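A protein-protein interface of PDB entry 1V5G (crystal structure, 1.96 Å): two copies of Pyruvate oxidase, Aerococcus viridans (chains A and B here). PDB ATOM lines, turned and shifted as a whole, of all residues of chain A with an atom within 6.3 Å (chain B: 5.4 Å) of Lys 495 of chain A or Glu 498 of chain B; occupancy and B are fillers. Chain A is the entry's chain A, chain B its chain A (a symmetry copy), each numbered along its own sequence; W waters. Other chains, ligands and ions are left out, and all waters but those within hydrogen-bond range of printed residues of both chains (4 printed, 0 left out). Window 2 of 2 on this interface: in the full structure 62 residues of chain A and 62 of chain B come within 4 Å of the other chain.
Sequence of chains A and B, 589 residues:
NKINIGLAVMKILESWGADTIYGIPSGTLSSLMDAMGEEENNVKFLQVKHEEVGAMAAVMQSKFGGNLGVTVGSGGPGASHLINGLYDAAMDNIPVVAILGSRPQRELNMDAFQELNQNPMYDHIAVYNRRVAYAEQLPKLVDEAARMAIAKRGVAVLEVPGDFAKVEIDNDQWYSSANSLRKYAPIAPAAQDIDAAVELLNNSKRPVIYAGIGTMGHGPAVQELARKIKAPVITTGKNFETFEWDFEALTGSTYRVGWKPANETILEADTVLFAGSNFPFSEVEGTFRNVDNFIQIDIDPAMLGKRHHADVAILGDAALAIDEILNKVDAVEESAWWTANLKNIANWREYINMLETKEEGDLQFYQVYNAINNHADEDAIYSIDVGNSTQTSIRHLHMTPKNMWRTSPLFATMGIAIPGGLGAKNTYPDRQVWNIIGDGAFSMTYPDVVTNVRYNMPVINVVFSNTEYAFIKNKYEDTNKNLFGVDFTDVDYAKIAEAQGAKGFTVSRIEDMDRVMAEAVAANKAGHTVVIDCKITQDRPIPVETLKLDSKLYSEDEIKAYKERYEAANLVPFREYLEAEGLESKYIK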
ATOM      1  N   ASP A 492     -16.989 -20.857 -21.753  1.00  0.00           N
ATOM      2  CA  ASP A 492     -17.834 -20.530 -20.619  1.00  0.00           C
ATOM      3  C   ASP A 492     -17.548 -19.127 -20.088  1.00  0.00           C
ATOM      4  O   ASP A 492     -16.800 -18.970 -19.124  1.00  0.00           O
ATOM      5  CB  ASP A 492     -17.595 -21.563 -19.519  1.00  0.00           C
ATOM      6  CG  ASP A 492     -18.614 -21.474 -18.411  1.00  0.00           C
ATOM      7  OD1 ASP A 492     -19.195 -20.386 -18.225  1.00  0.00           O
ATOM      8  OD2 ASP A 492     -18.814 -22.494 -17.723  1.00  0.00           O
ATOM      9  N   TYR A 493     -18.146 -18.109 -20.704  1.00  0.00           N
ATOM     10  CA  TYR A 493     -17.918 -16.730 -20.268  1.00  0.00           C
ATOM     11  C   TYR A 493     -18.386 -16.462 -18.844  1.00  0.00           C
ATOM     12  O   TYR A 493     -17.813 -15.628 -18.149  1.00  0.00           O
ATOM     13  CB  TYR A 493     -18.596 -15.745 -21.226  1.00  0.00           C
ATOM     14  CG  TYR A 493     -18.105 -15.879 -22.642  1.00  0.00           C
ATOM     15  CD1 TYR A 493     -18.974 -16.247 -23.665  1.00  0.00           C
ATOM     16  CD2 TYR A 493     -16.755 -15.704 -22.951  1.00  0.00           C
ATOM     17  CE1 TYR A 493     -18.513 -16.446 -24.957  1.00  0.00           C
ATOM     18  CE2 TYR A 493     -16.283 -15.900 -24.238  1.00  0.00           C
ATOM     19  CZ  TYR A 493     -17.168 -16.275 -25.236  1.00  0.00           C
ATOM     20  OH  TYR A 493     -16.708 -16.516 -26.509  1.00  0.00           O
ATOM     21  N   ALA A 494     -19.426 -17.163 -18.408  1.00  0.00           N
ATOM     22  CA  ALA A 494     -19.931 -16.979 -17.051  1.00  0.00           C
ATOM     23  C   ALA A 494     -18.844 -17.393 -16.059  1.00  0.00           C
ATOM     24  O   ALA A 494     -18.627 -16.738 -15.038  1.00  0.00           O
ATOM     25  CB  ALA A 494     -21.199 -17.817 -16.839  1.00  0.00           C
ATOM     26  N   LYS A 495     -18.154 -18.483 -16.373  1.00  0.00           N
ATOM     27  CA  LYS A 495     -17.085 -18.990 -15.521  1.00  0.00           C
ATOM     28  C   LYS A 495     -15.888 -18.039 -15.535  1.00  0.00           C
ATOM     29  O   LYS A 495     -15.189 -17.885 -14.533  1.00  0.00           O
ATOM     30  CB  LYS A 495     -16.657 -20.380 -15.997  1.00  0.00           C
ATOM     31  CG  LYS A 495     -15.673 -21.078 -15.079  1.00  0.00           C
ATOM     32  CD  LYS A 495     -15.422 -22.508 -15.532  1.00  0.00           C
ATOM     33  CE  LYS A 495     -14.460 -23.216 -14.595  1.00  0.00           C
ATOM     34  NZ  LYS A 495     -14.183 -24.619 -15.022  1.00  0.00           N
ATOM     35  N   ILE A 496     -15.648 -17.406 -16.676  1.00  0.00           N
ATOM     36  CA  ILE A 496     -14.542 -16.465 -16.788  1.00  0.00           C
ATOM     37  C   ILE A 496     -14.842 -15.272 -15.888  1.00  0.00           C
ATOM     38  O   ILE A 496     -13.971 -14.797 -15.161  1.00  0.00           O
ATOM     39  CB  ILE A 496     -14.346 -16.010 -18.254  1.00  0.00           C
ATOM     40  CG1 ILE A 496     -13.893 -17.209 -19.096  1.00  0.00           C
ATOM     41  CG2 ILE A 496     -13.324 -14.873 -18.327  1.00  0.00           C
ATOM     42  CD1 ILE A 496     -13.695 -16.914 -20.582  1.00  0.00           C
ATOM     43  N   ALA A 497     -16.087 -14.810 -15.919  1.00  0.00           N
ATOM     44  CA  ALA A 497     -16.511 -13.684 -15.095  1.00  0.00           C
ATOM     45  C   ALA A 497     -16.313 -13.980 -13.611  1.00  0.00           C
ATOM     46  O   ALA A 497     -15.878 -13.117 -12.850  1.00  0.00           O
ATOM     47  CB  ALA A 497     -17.971 -13.360 -15.366  1.00  0.00           C
ATOM     48  N   GLU A 498     -16.640 -15.201 -13.202  1.00  0.00           N
ATOM     49  CA  GLU A 498     -16.485 -15.593 -11.807  1.00  0.00           C
ATOM     50  C   GLU A 498     -15.017 -15.545 -11.414  1.00  0.00           C
ATOM     51  O   GLU A 498     -14.677 -15.097 -10.321  1.00  0.00           O
ATOM     52  CB  GLU A 498     -17.036 -17.008 -11.581  1.00  0.00           C
ATOM     53  CG  GLU A 498     -18.547 -17.135 -11.781  1.00  0.00           C
ATOM     54  CD  GLU A 498     -19.354 -16.429 -10.696  1.00  0.00           C
ATOM     55  OE1 GLU A 498     -20.582 -16.256 -10.874  1.00  0.00           O
ATOM     56  OE2 GLU A 498     -18.762 -16.055  -9.658  1.00  0.00           O
ATOM     57  N   ALA A 499     -14.151 -16.000 -12.315  1.00  0.00           N
ATOM     58  CA  ALA A 499     -12.714 -16.016 -12.057  1.00  0.00           C
ATOM     59  C   ALA A 499     -12.170 -14.604 -11.902  1.00  0.00           C
ATOM     60  O   ALA A 499     -11.126 -14.403 -11.281  1.00  0.00           O
ATOM     61  CB  ALA A 499     -11.989 -16.723 -13.188  1.00  0.00           C
ATOM     62  N   GLN A 500     -12.892 -13.635 -12.463  1.00  0.00           N
ATOM     63  CA  GLN A 500     -12.495 -12.233 -12.416  1.00  0.00           C
ATOM     64  C   GLN A 500     -13.126 -11.449 -11.263  1.00  0.00           C
ATOM     65  O   GLN A 500     -12.873 -10.256 -11.119  1.00  0.00           O
ATOM     66  CB  GLN A 500     -12.853 -11.545 -13.739  1.00  0.00           C
ATOM     67  CG  GLN A 500     -12.242 -12.192 -14.968  1.00  0.00           C
ATOM     68  CD  GLN A 500     -12.797 -11.618 -16.257  1.00  0.00           C
ATOM     69  OE1 GLN A 500     -14.009 -11.513 -16.424  1.00  0.00           O
ATOM     70  NE2 GLN A 500     -11.912 -11.252 -17.176  1.00  0.00           N
ATOM     71  N   GLY A 504     -21.355 -14.421 -12.857  1.00  0.00           N
ATOM     72  CA  GLY A 504     -21.709 -14.961 -14.153  1.00  0.00           C
ATOM     73  C   GLY A 504     -23.010 -15.734 -14.192  1.00  0.00           C
ATOM     74  O   GLY A 504     -23.392 -16.394 -13.219  1.00  0.00           O
ATOM     75  N   THR A 506     -25.603 -18.062 -17.101  1.00  0.00           N
ATOM     76  CA  THR A 506     -25.661 -18.762 -18.372  1.00  0.00           C
ATOM     77  C   THR A 506     -27.129 -19.042 -18.637  1.00  0.00           C
ATOM     78  O   THR A 506     -27.851 -19.483 -17.744  1.00  0.00           O
ATOM     79  CB  THR A 506     -24.900 -20.099 -18.316  1.00  0.00           C
ATOM     80  OG1 THR A 506     -23.541 -19.858 -17.937  1.00  0.00           O
ATOM     81  CG2 THR A 506     -24.930 -20.788 -19.676  1.00  0.00           C
ATOM     82  N   ASP A 533     -24.123 -14.824 -20.021  1.00  0.00           N
ATOM     83  CA  ASP A 533     -23.716 -15.571 -21.209  1.00  0.00           C
ATOM     84  C   ASP A 533     -24.955 -16.132 -21.900  1.00  0.00           C
ATOM     85  O   ASP A 533     -25.484 -17.173 -21.506  1.00  0.00           O
ATOM     86  CB  ASP A 533     -22.775 -16.715 -20.818  1.00  0.00           C
ATOM     87  CG  ASP A 533     -22.063 -17.319 -22.012  1.00  0.00           C
ATOM     88  OD1 ASP A 533     -22.404 -16.953 -23.160  1.00  0.00           O
ATOM     89  OD2 ASP A 533     -21.163 -18.160 -21.802  1.00  0.00           O
ATOM     90  N   TYR B 493      -6.583 -17.445 -13.179  1.00  0.00           N
ATOM     91  CA  TYR B 493      -6.252 -17.784 -14.564  1.00  0.00           C
ATOM     92  C   TYR B 493      -6.434 -19.262 -14.883  1.00  0.00           C
ATOM     93  O   TYR B 493      -6.751 -19.618 -16.015  1.00  0.00           O
ATOM     94  CB  TYR B 493      -4.818 -17.359 -14.894  1.00  0.00           C
ATOM     95  CG  TYR B 493      -4.589 -15.885 -14.701  1.00  0.00           C
ATOM     96  CD1 TYR B 493      -3.670 -15.422 -13.765  1.00  0.00           C
ATOM     97  CD2 TYR B 493      -5.341 -14.946 -15.411  1.00  0.00           C
ATOM     98  CE1 TYR B 493      -3.509 -14.066 -13.530  1.00  0.00           C
ATOM     99  CE2 TYR B 493      -5.189 -13.588 -15.184  1.00  0.00           C
ATOM    100  CZ  TYR B 493      -4.273 -13.155 -14.238  1.00  0.00           C
ATOM    101  OH  TYR B 493      -4.142 -11.813 -13.971  1.00  0.00           O
ATOM    102  N   ALA B 494      -6.232 -20.123 -13.893  1.00  0.00           N
ATOM    103  CA  ALA B 494      -6.399 -21.557 -14.109  1.00  0.00           C
ATOM    104  C   ALA B 494      -7.858 -21.837 -14.467  1.00  0.00           C
ATOM    105  O   ALA B 494      -8.156 -22.643 -15.350  1.00  0.00           O
ATOM    106  CB  ALA B 494      -5.998 -22.332 -12.847  1.00  0.00           C
ATOM    107  N   LYS B 495      -8.767 -21.155 -13.780  1.00  0.00           N
ATOM    108  CA  LYS B 495     -10.196 -21.318 -14.020  1.00  0.00           C
ATOM    109  C   LYS B 495     -10.580 -20.755 -15.389  1.00  0.00           C
ATOM    110  O   LYS B 495     -11.474 -21.272 -16.059  1.00  0.00           O
ATOM    111  CB  LYS B 495     -10.991 -20.611 -12.920  1.00  0.00           C
ATOM    112  CG  LYS B 495     -12.485 -20.864 -12.970  1.00  0.00           C
ATOM    113  CD  LYS B 495     -13.182 -20.264 -11.759  1.00  0.00           C
ATOM    114  CE  LYS B 495     -14.674 -20.543 -11.794  1.00  0.00           C
ATOM    115  NZ  LYS B 495     -15.388 -19.955 -10.624  1.00  0.00           N
ATOM    116  N   ILE B 496      -9.908 -19.688 -15.800  1.00  0.00           N
ATOM    117  CA  ILE B 496     -10.185 -19.087 -17.097  1.00  0.00           C
ATOM    118  C   ILE B 496      -9.778 -20.081 -18.178  1.00  0.00           C
ATOM    119  O   ILE B 496     -10.509 -20.293 -19.145  1.00  0.00           O
ATOM    120  CB  ILE B 496      -9.420 -17.752 -17.266  1.00  0.00           C
ATOM    121  CG1 ILE B 496      -9.968 -16.729 -16.263  1.00  0.00           C
ATOM    122  CG2 ILE B 496      -9.556 -17.237 -18.700  1.00  0.00           C
ATOM    123  CD1 ILE B 496      -9.276 -15.366 -16.290  1.00  0.00           C
ATOM    124  N   ALA B 497      -8.624 -20.711 -17.993  1.00  0.00           N
ATOM    125  CA  ALA B 497      -8.126 -21.699 -18.943  1.00  0.00           C
ATOM    126  C   ALA B 497      -9.106 -22.859 -19.097  1.00  0.00           C
ATOM    127  O   ALA B 497      -9.338 -23.344 -20.205  1.00  0.00           O
ATOM    128  CB  ALA B 497      -6.773 -22.224 -18.490  1.00  0.00           C
ATOM    129  N   GLU B 498      -9.674 -23.307 -17.983  1.00  0.00           N
ATOM    130  CA  GLU B 498     -10.630 -24.406 -18.016  1.00  0.00           C
ATOM    131  C   GLU B 498     -11.857 -24.005 -18.820  1.00  0.00           C
ATOM    132  O   GLU B 498     -12.383 -24.799 -19.597  1.00  0.00           O
ATOM    133  CB  GLU B 498     -11.049 -24.798 -16.593  1.00  0.00           C
ATOM    134  CG  GLU B 498      -9.920 -25.384 -15.742  1.00  0.00           C
ATOM    135  CD  GLU B 498      -9.476 -26.766 -16.208  1.00  0.00           C
ATOM    136  OE1 GLU B 498      -8.413 -27.244 -15.752  1.00  0.00           O
ATOM    137  OE2 GLU B 498     -10.199 -27.381 -17.026  1.00  0.00           O
ATOM    138  N   ALA B 499     -12.301 -22.765 -18.636  1.00  0.00           N
ATOM    139  CA  ALA B 499     -13.475 -22.259 -19.341  1.00  0.00           C
ATOM    140  C   ALA B 499     -13.229 -22.198 -20.841  1.00  0.00           C
ATOM    141  O   ALA B 499     -14.175 -22.216 -21.629  1.00  0.00           O
ATOM    142  CB  ALA B 499     -13.838 -20.878 -18.826  1.00  0.00           C
ATOM    143  N   GLN B 500     -11.953 -22.137 -21.221  1.00  0.00           N
ATOM    144  CA  GLN B 500     -11.555 -22.057 -22.621  1.00  0.00           C
ATOM    145  C   GLN B 500     -11.232 -23.414 -23.251  1.00  0.00           C
ATOM    146  O   GLN B 500     -10.879 -23.479 -24.426  1.00  0.00           O
ATOM    147  CB  GLN B 500     -10.335 -21.139 -22.765  1.00  0.00           C
ATOM    148  CG  GLN B 500     -10.539 -19.735 -22.226  1.00  0.00           C
ATOM    149  CD  GLN B 500      -9.249 -18.939 -22.189  1.00  0.00           C
ATOM    150  OE1 GLN B 500      -8.236 -19.415 -21.683  1.00  0.00           O
ATOM    151  NE2 GLN B 500      -9.284 -17.721 -22.716  1.00  0.00           N
ATOM    152  N   GLY B 501     -11.338 -24.490 -22.476  1.00  0.00           N
ATOM    153  CA  GLY B 501     -11.050 -25.808 -23.016  1.00  0.00           C
ATOM    154  C   GLY B 501      -9.606 -26.204 -22.791  1.00  0.00           C
ATOM    155  O   GLY B 501      -9.119 -27.199 -23.329  1.00  0.00           O
ATOM    156  N   ALA B 502      -8.911 -25.409 -21.990  1.00  0.00           N
ATOM    157  CA  ALA B 502      -7.518 -25.678 -21.678  1.00  0.00           C
ATOM    158  C   ALA B 502      -7.451 -26.270 -20.277  1.00  0.00           C
ATOM    159  O   ALA B 502      -8.444 -26.294 -19.556  1.00  0.00           O
ATOM    160  CB  ALA B 502      -6.713 -24.391 -21.751  1.00  0.00           C
ATOM    161  N   LYS B 503      -6.281 -26.760 -19.900  1.00  0.00           N
ATOM    162  CA  LYS B 503      -6.088 -27.348 -18.582  1.00  0.00           C
ATOM    163  C   LYS B 503      -5.389 -26.338 -17.687  1.00  0.00           C
ATOM    164  O   LYS B 503      -4.311 -25.849 -18.016  1.00  0.00           O
ATOM    165  CB  LYS B 503      -5.248 -28.623 -18.697  1.00  0.00           C
ATOM    166  CG  LYS B 503      -4.790 -29.206 -17.370  1.00  0.00           C
ATOM    167  CD  LYS B 503      -5.951 -29.599 -16.468  1.00  0.00           C
ATOM    168  CE  LYS B 503      -5.439 -30.208 -15.170  1.00  0.00           C
ATOM    169  NZ  LYS B 503      -6.538 -30.544 -14.225  1.00  0.00           N
ATOM    170  N   GLY B 504      -6.005 -26.034 -16.550  1.00  0.00           N
ATOM    171  CA  GLY B 504      -5.421 -25.067 -15.644  1.00  0.00           C
ATOM    172  C   GLY B 504      -4.847 -25.647 -14.369  1.00  0.00           C
ATOM    173  O   GLY B 504      -5.352 -26.639 -13.833  1.00  0.00           O
HETATM  174  O   HOH W   1     -15.214 -17.547  -8.845  1.00  0.00           O
HETATM  175  O   HOH W   2     -13.913 -26.200 -17.556  1.00  0.00           O
HETATM  176  O   HOH W   3     -13.193 -27.870 -15.734  1.00  0.00           O
HETATM  177  O   HOH W   4     -17.425 -18.654  -8.130  1.00  0.00           O
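N of Asp 492 of chain A is in hydrogen-bond range of O of Ala 499 of chain B (3.1 Å).
The side-chain carboxylate of Glu 498 of chain B is in hydrogen-bond range of the backbone NH of Gly 504 of chain B (2.8 Å). The backbone NH (N) of Ala 494 of chain A sits close to the side-chain carboxylate (OD1) of Asp 492 of chain A. The side-chain carboxylate of Asp 492 of chain A lies within hydrogen-bond range of the backbone NH of Lys 495 of chain A (2.9 Å). The backbone NH (N) of Gly 504 of chain A sits at hydrogen-bond distance from the side-chain carboxylate (OE1) of Glu 498 of chain A, 2.8 Å away.
Among the printed residues, merely in contact across the chains: Lys 495 of chain A with Lys 495 of chain B (3.5 Å), Glu 498 of chain A with Lys 495 of chain B (3.5 Å), Lys 495 of chain A with Glu 498 of chain B (3.5 Å), Ile 496 of chain A with Ala 499 of chain B (3.7 Å) and Ala 499 of chain A with Ile 496 of chain B (3.7 Å).
Printed residues of chain B within 4 Å of Asp 492 of chain A: Ala 499 (3.1 Å). Printed residues of chain B within 4 Å of Lys 495 of chain A: Lys 495 (3.5 Å) and Glu 498 (3.5 Å). Printed residues of chain B within 4 Å of Ile 496 of chain A: Ala 499 (3.7 Å). Gln 500 of chain A touches none of the printed residues of chain B. The nearest printed residue of chain B that does not touch Ala 499 of chain A is Lys 495 of chain B (4.0005 Å).
Along chain A the printed residues that touch a printed residue of chain B span positions 492 to 499. Hydrophobic or aromatic side chains of chain B that line the printed part of chain A: Ile 496 and Ala 499. Among the printed residues, no Asp or Glu carboxylate lies within 4 Å of a Lys or Arg side-chain nitrogen of the other chain.
Lys 495 of chain B touches its own counterpart, Lys 495 of chain A. Lys 495 of chain A touches Glu 498 of chain B, and with the chains exchanged Glu 498 of chain A touches Lys 495 of chain B. Ile 496 of chain A touches Ala 499 of chain B, and with the chains exchanged Ala 499 of chain A touches Ile 496 of chain B. Positions printed for both chains: 493, 494, 495, 496, 497, 498, 499, 500 and 504. Of the 6 pairs that touch across the chains among the printed residues, 5 have their exchanged pair printed and touching as well.
Water W2 lies within hydrogen-bond range of the backbone carbonyl oxygen (O) of Glu 498 of chain B (2.9 Å) and the side-chain amino group (NZ) of Lys 495 of chain A (3.0 Å). Water W1 bridges O of Glu 498 of chain A (2.9 Å) and NZ of Lys 495 of chain B (3.0 Å). Water W3 bridges OE2 of Glu 498 of chain B (3.3 Å) and NZ of Lys 495 of chain A (3.5 Å). Water W4 lies within hydrogen-bond range of OE2 of Glu 498 of chain A and NZ of Lys 495 of chain B.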
